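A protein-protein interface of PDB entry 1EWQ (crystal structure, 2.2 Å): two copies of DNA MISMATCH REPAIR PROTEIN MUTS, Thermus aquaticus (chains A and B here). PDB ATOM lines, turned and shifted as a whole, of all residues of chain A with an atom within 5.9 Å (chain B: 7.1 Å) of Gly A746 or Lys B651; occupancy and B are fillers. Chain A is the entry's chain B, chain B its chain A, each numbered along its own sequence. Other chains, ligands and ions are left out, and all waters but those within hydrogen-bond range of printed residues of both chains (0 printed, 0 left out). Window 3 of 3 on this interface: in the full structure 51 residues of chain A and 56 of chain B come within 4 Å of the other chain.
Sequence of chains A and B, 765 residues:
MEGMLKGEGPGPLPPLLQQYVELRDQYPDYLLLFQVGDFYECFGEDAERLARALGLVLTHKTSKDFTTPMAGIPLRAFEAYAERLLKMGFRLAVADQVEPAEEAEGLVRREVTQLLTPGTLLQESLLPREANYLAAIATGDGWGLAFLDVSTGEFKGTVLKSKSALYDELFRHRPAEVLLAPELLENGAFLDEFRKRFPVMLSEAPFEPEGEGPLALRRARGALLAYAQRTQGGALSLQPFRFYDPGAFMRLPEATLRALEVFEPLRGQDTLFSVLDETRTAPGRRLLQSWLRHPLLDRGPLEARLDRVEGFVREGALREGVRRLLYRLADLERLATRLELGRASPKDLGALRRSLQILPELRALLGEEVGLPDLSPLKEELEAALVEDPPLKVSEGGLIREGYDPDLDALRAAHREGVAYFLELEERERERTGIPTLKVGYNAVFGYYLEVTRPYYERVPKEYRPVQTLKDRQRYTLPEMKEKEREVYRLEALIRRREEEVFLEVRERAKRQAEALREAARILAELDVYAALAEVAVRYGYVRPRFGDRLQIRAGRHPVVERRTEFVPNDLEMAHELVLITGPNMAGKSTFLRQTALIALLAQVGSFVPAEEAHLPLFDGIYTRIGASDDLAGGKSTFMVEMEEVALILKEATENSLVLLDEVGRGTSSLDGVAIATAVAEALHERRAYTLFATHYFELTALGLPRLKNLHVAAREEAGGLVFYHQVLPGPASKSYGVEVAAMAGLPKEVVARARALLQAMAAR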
ATOM      1  N   VAL A 741     -27.747   7.949 -20.023  1.00  0.00           N
ATOM      2  CA  VAL A 741     -27.760   9.392 -19.838  1.00  0.00           C
ATOM      3  C   VAL A 741     -26.325   9.900 -19.848  1.00  0.00           C
ATOM      4  O   VAL A 741     -26.027  10.952 -20.422  1.00  0.00           O
ATOM      5  CB  VAL A 741     -28.438   9.764 -18.504  1.00  0.00           C
ATOM      6  CG1 VAL A 741     -28.266  11.256 -18.212  1.00  0.00           C
ATOM      7  CG2 VAL A 741     -29.916   9.400 -18.569  1.00  0.00           C
ATOM      8  N   ALA A 742     -25.437   9.142 -19.212  1.00  0.00           N
ATOM      9  CA  ALA A 742     -24.030   9.503 -19.150  1.00  0.00           C
ATOM     10  C   ALA A 742     -23.480   9.507 -20.567  1.00  0.00           C
ATOM     11  O   ALA A 742     -22.711  10.389 -20.954  1.00  0.00           O
ATOM     12  CB  ALA A 742     -23.270   8.501 -18.289  1.00  0.00           C
ATOM     13  N   ALA A 743     -23.883   8.511 -21.346  1.00  0.00           N
ATOM     14  CA  ALA A 743     -23.432   8.413 -22.722  1.00  0.00           C
ATOM     15  C   ALA A 743     -23.928   9.634 -23.476  1.00  0.00           C
ATOM     16  O   ALA A 743     -23.236  10.170 -24.336  1.00  0.00           O
ATOM     17  CB  ALA A 743     -23.978   7.146 -23.360  1.00  0.00           C
ATOM     18  N   MET A 744     -25.133  10.074 -23.131  1.00  0.00           N
ATOM     19  CA  MET A 744     -25.747  11.226 -23.779  1.00  0.00           C
ATOM     20  C   MET A 744     -25.105  12.529 -23.313  1.00  0.00           C
ATOM     21  O   MET A 744     -25.176  13.548 -23.999  1.00  0.00           O
ATOM     22  CB  MET A 744     -27.246  11.249 -23.473  1.00  0.00           C
ATOM     23  CG  MET A 744     -28.079  12.098 -24.428  1.00  0.00           C
ATOM     24  SD  MET A 744     -29.936  12.256 -23.856  1.00  0.00           S
ATOM     25  CE  MET A 744     -30.089  10.520 -23.019  1.00  0.00           C
ATOM     26  N   ALA A 745     -24.479  12.487 -22.143  1.00  0.00           N
ATOM     27  CA  ALA A 745     -23.829  13.664 -21.579  1.00  0.00           C
ATOM     28  C   ALA A 745     -22.485  13.950 -22.243  1.00  0.00           C
ATOM     29  O   ALA A 745     -21.884  15.000 -22.011  1.00  0.00           O
ATOM     30  CB  ALA A 745     -23.648  13.487 -20.072  1.00  0.00           C
ATOM     31  N   GLY A 746     -22.010  13.018 -23.065  1.00  0.00           N
ATOM     32  CA  GLY A 746     -20.747  13.227 -23.751  1.00  0.00           C
ATOM     33  C   GLY A 746     -19.550  12.562 -23.104  1.00  0.00           C
ATOM     34  O   GLY A 746     -18.403  12.886 -23.416  1.00  0.00           O
ATOM     35  N   LEU A 747     -19.819  11.633 -22.196  1.00  0.00           N
ATOM     36  CA  LEU A 747     -18.768  10.897 -21.504  1.00  0.00           C
ATOM     37  C   LEU A 747     -18.096   9.997 -22.551  1.00  0.00           C
ATOM     38  O   LEU A 747     -18.777   9.355 -23.343  1.00  0.00           O
ATOM     39  CB  LEU A 747     -19.391  10.046 -20.393  1.00  0.00           C
ATOM     40  CG  LEU A 747     -18.665   9.894 -19.051  1.00  0.00           C
ATOM     41  CD1 LEU A 747     -17.270   9.350 -19.276  1.00  0.00           C
ATOM     42  CD2 LEU A 747     -18.590  11.237 -18.347  1.00  0.00           C
ATOM     43  N   PRO A 748     -16.753   9.948 -22.572  1.00  0.00           N
ATOM     44  CA  PRO A 748     -16.030   9.113 -23.542  1.00  0.00           C
ATOM     45  C   PRO A 748     -16.659   7.741 -23.793  1.00  0.00           C
ATOM     46  O   PRO A 748     -17.055   7.045 -22.855  1.00  0.00           O
ATOM     47  CB  PRO A 748     -14.640   9.013 -22.929  1.00  0.00           C
ATOM     48  CG  PRO A 748     -14.458  10.383 -22.342  1.00  0.00           C
ATOM     49  CD  PRO A 748     -15.809  10.665 -21.693  1.00  0.00           C
ATOM     50  N   MET B 643     -22.548  14.712 -15.133  1.00  0.00           N
ATOM     51  CA  MET B 643     -21.901  13.860 -16.125  1.00  0.00           C
ATOM     52  C   MET B 643     -21.276  14.724 -17.219  1.00  0.00           C
ATOM     53  O   MET B 643     -20.214  14.393 -17.743  1.00  0.00           O
ATOM     54  CB  MET B 643     -22.891  12.864 -16.746  1.00  0.00           C
ATOM     55  CG  MET B 643     -23.326  11.748 -15.815  1.00  0.00           C
ATOM     56  SD  MET B 643     -21.844  10.687 -15.181  1.00  0.00           S
ATOM     57  CE  MET B 643     -21.567  11.525 -13.460  1.00  0.00           C
ATOM     58  N   GLU B 644     -21.933  15.829 -17.565  1.00  0.00           N
ATOM     59  CA  GLU B 644     -21.397  16.733 -18.580  1.00  0.00           C
ATOM     60  C   GLU B 644     -20.074  17.299 -18.077  1.00  0.00           C
ATOM     61  O   GLU B 644     -19.088  17.338 -18.810  1.00  0.00           O
ATOM     62  CB  GLU B 644     -22.368  17.890 -18.862  1.00  0.00           C
ATOM     63  CG  GLU B 644     -23.538  17.521 -19.750  1.00  0.00           C
ATOM     64  CD  GLU B 644     -24.452  18.704 -20.049  1.00  0.00           C
ATOM     65  OE1 GLU B 644     -25.314  18.573 -20.935  1.00  0.00           O
ATOM     66  OE2 GLU B 644     -24.318  19.759 -19.399  1.00  0.00           O
ATOM     67  N   GLU B 645     -20.055  17.738 -16.822  1.00  0.00           N
ATOM     68  CA  GLU B 645     -18.835  18.292 -16.250  1.00  0.00           C
ATOM     69  C   GLU B 645     -17.712  17.249 -16.245  1.00  0.00           C
ATOM     70  O   GLU B 645     -16.568  17.561 -16.572  1.00  0.00           O
ATOM     71  CB  GLU B 645     -19.096  18.793 -14.830  1.00  0.00           C
ATOM     72  CG  GLU B 645     -19.988  20.024 -14.760  1.00  0.00           C
ATOM     73  CD  GLU B 645     -20.374  20.387 -13.327  1.00  0.00           C
ATOM     74  OE1 GLU B 645     -19.482  20.387 -12.439  1.00  0.00           O
ATOM     75  OE2 GLU B 645     -21.568  20.691 -13.098  1.00  0.00           O
ATOM     76  N   VAL B 646     -18.046  16.016 -15.874  1.00  0.00           N
ATOM     77  CA  VAL B 646     -17.065  14.937 -15.851  1.00  0.00           C
ATOM     78  C   VAL B 646     -16.462  14.746 -17.242  1.00  0.00           C
ATOM     79  O   VAL B 646     -15.253  14.572 -17.380  1.00  0.00           O
ATOM     80  CB  VAL B 646     -17.699  13.603 -15.379  1.00  0.00           C
ATOM     81  CG1 VAL B 646     -16.731  12.447 -15.589  1.00  0.00           C
ATOM     82  CG2 VAL B 646     -18.058  13.703 -13.903  1.00  0.00           C
ATOM     83  N   ALA B 647     -17.310  14.782 -18.269  1.00  0.00           N
ATOM     84  CA  ALA B 647     -16.851  14.631 -19.645  1.00  0.00           C
ATOM     85  C   ALA B 647     -15.814  15.697 -19.972  1.00  0.00           C
ATOM     86  O   ALA B 647     -14.741  15.378 -20.464  1.00  0.00           O
ATOM     87  CB  ALA B 647     -18.021  14.729 -20.611  1.00  0.00           C
ATOM     88  N   LEU B 648     -16.126  16.962 -19.710  1.00  0.00           N
ATOM     89  CA  LEU B 648     -15.166  18.018 -19.992  1.00  0.00           C
ATOM     90  C   LEU B 648     -13.854  17.712 -19.284  1.00  0.00           C
ATOM     91  O   LEU B 648     -12.772  17.863 -19.863  1.00  0.00           O
ATOM     92  CB  LEU B 648     -15.683  19.386 -19.530  1.00  0.00           C
ATOM     93  CG  LEU B 648     -16.666  20.127 -20.447  1.00  0.00           C
ATOM     94  CD1 LEU B 648     -16.964  21.490 -19.857  1.00  0.00           C
ATOM     95  CD2 LEU B 648     -16.068  20.288 -21.856  1.00  0.00           C
ATOM     96  N   ILE B 649     -13.952  17.265 -18.034  1.00  0.00           N
ATOM     97  CA  ILE B 649     -12.759  16.945 -17.266  1.00  0.00           C
ATOM     98  C   ILE B 649     -11.940  15.826 -17.908  1.00  0.00           C
ATOM     99  O   ILE B 649     -10.723  15.937 -18.017  1.00  0.00           O
ATOM    100  CB  ILE B 649     -13.119  16.562 -15.820  1.00  0.00           C
ATOM    101  CG1 ILE B 649     -13.720  17.775 -15.110  1.00  0.00           C
ATOM    102  CG2 ILE B 649     -11.882  16.077 -15.084  1.00  0.00           C
ATOM    103  CD1 ILE B 649     -14.227  17.502 -13.702  1.00  0.00           C
ATOM    104  N   LEU B 650     -12.606  14.759 -18.346  1.00  0.00           N
ATOM    105  CA  LEU B 650     -11.917  13.626 -18.964  1.00  0.00           C
ATOM    106  C   LEU B 650     -11.246  13.982 -20.277  1.00  0.00           C
ATOM    107  O   LEU B 650     -10.237  13.387 -20.644  1.00  0.00           O
ATOM    108  CB  LEU B 650     -12.893  12.466 -19.198  1.00  0.00           C
ATOM    109  CG  LEU B 650     -13.403  11.791 -17.923  1.00  0.00           C
ATOM    110  CD1 LEU B 650     -14.499  10.812 -18.256  1.00  0.00           C
ATOM    111  CD2 LEU B 650     -12.255  11.094 -17.227  1.00  0.00           C
ATOM    112  N   LYS B 651     -11.804  14.959 -20.979  1.00  0.00           N
ATOM    113  CA  LYS B 651     -11.264  15.379 -22.260  1.00  0.00           C
ATOM    114  C   LYS B 651     -10.123  16.391 -22.153  1.00  0.00           C
ATOM    115  O   LYS B 651      -9.296  16.494 -23.054  1.00  0.00           O
ATOM    116  CB  LYS B 651     -12.399  15.935 -23.122  1.00  0.00           C
ATOM    117  CG  LYS B 651     -13.436  14.875 -23.476  1.00  0.00           C
ATOM    118  CD  LYS B 651     -14.648  15.450 -24.196  1.00  0.00           C
ATOM    119  CE  LYS B 651     -15.748  14.388 -24.320  1.00  0.00           C
ATOM    120  NZ  LYS B 651     -17.052  14.966 -24.774  1.00  0.00           N
ATOM    121  N   GLU B 652     -10.065  17.134 -21.055  1.00  0.00           N
ATOM    122  CA  GLU B 652      -9.003  18.117 -20.888  1.00  0.00           C
ATOM    123  C   GLU B 652      -7.912  17.665 -19.921  1.00  0.00           C
ATOM    124  O   GLU B 652      -6.773  18.101 -20.041  1.00  0.00           O
ATOM    125  CB  GLU B 652      -9.593  19.466 -20.445  1.00  0.00           C
ATOM    126  CG  GLU B 652     -10.240  19.501 -19.053  1.00  0.00           C
ATOM    127  CD  GLU B 652     -11.157  20.723 -18.844  1.00  0.00           C
ATOM    128  OE1 GLU B 652     -11.108  21.675 -19.661  1.00  0.00           O
ATOM    129  OE2 GLU B 652     -11.925  20.731 -17.853  1.00  0.00           O
ATOM    130  N   ALA B 653      -8.253  16.773 -18.991  1.00  0.00           N
ATOM    131  CA  ALA B 653      -7.303  16.277 -17.988  1.00  0.00           C
ATOM    132  C   ALA B 653      -6.104  15.518 -18.543  1.00  0.00           C
ATOM    133  O   ALA B 653      -6.234  14.651 -19.407  1.00  0.00           O
ATOM    134  CB  ALA B 653      -8.021  15.405 -16.981  1.00  0.00           C
ATOM    135  N   THR B 654      -4.939  15.820 -17.982  1.00  0.00           N
ATOM    136  CA  THR B 654      -3.681  15.222 -18.394  1.00  0.00           C
ATOM    137  C   THR B 654      -2.986  14.546 -17.201  1.00  0.00           C
ATOM    138  O   THR B 654      -3.492  14.602 -16.081  1.00  0.00           O
ATOM    139  CB  THR B 654      -2.799  16.339 -18.993  1.00  0.00           C
ATOM    140  OG1 THR B 654      -2.494  16.022 -20.349  1.00  0.00           O
ATOM    141  CG2 THR B 654      -1.534  16.554 -18.188  1.00  0.00           C
ATOM    142  N   ARG B 687      -5.277   7.776 -16.816  1.00  0.00           N
ATOM    143  CA  ARG B 687      -4.781   9.090 -17.221  1.00  0.00           C
ATOM    144  C   ARG B 687      -3.545   9.484 -16.416  1.00  0.00           C
ATOM    145  O   ARG B 687      -2.714  10.256 -16.885  1.00  0.00           O
ATOM    146  CB  ARG B 687      -5.874  10.156 -17.040  1.00  0.00           C
ATOM    147  CG  ARG B 687      -5.546  11.508 -17.669  1.00  0.00           C
ATOM    148  CD  ARG B 687      -5.347  11.360 -19.181  1.00  0.00           C
ATOM    149  NE  ARG B 687      -6.489  10.699 -19.808  1.00  0.00           N
ATOM    150  CZ  ARG B 687      -7.627  11.308 -20.133  1.00  0.00           C
ATOM    151  NH1 ARG B 687      -7.788  12.606 -19.906  1.00  0.00           N
ATOM    152  NH2 ARG B 687      -8.616  10.610 -20.675  1.00  0.00           N
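The backbone carbonyl oxygen of Gly A746 sits at hydrogen-bond distance from the side-chain amino group of Lys B651, 2.8 Å away.
N of Leu A747 sits close to O of Ala A742 (3.4 Å). The backbone carbonyl oxygen (O) of Leu B650 sits at hydrogen-bond distance from the guanidinium group (NH1) of Arg B687.
Among the printed residues, pairs that only touch across the chains: Leu A747 with Leu B650, Gly A746 with Ala B647, Ala A745 with Met B643, Leu A747 with Val B646, Leu A747 with Met B643, Pro A748 with Leu B650, Ala A745 with Glu B644 and Leu A747 with Ala B647.
Lys B651 touches just one residue of chain A: Gly A746. Of the printed residues of chain B, Ala A745 touches Met B643 (3.5 Å) and Glu B644 (3.8 Å). Of the printed residues of chain A, Glu B644 touches Ala A745 (3.8 Å). Printed residues of chain A within 4 Å of Leu B650: Leu A747 (3.3 Å) and Pro A748 (3.7 Å). Of the printed residues of chain A, Ala B647 touches Gly A746 and Leu A747. The nearest residue of chain B that does not touch Gly A746 is Met B643 (5.7 Å).
Of the 13 printed residues of chain B, 6 touch a printed residue of chain A. Among the printed residues, 9 pairs touch across the chains. Among the printed residues, no Asp or Glu carboxylate lies within 4 Å of a Lys or Arg side-chain nitrogen of the other chain.
No position is printed for both chains. Of the 9 pairs that touch across the chains among the printed residues, none has its exchanged pair printed and touching as well.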
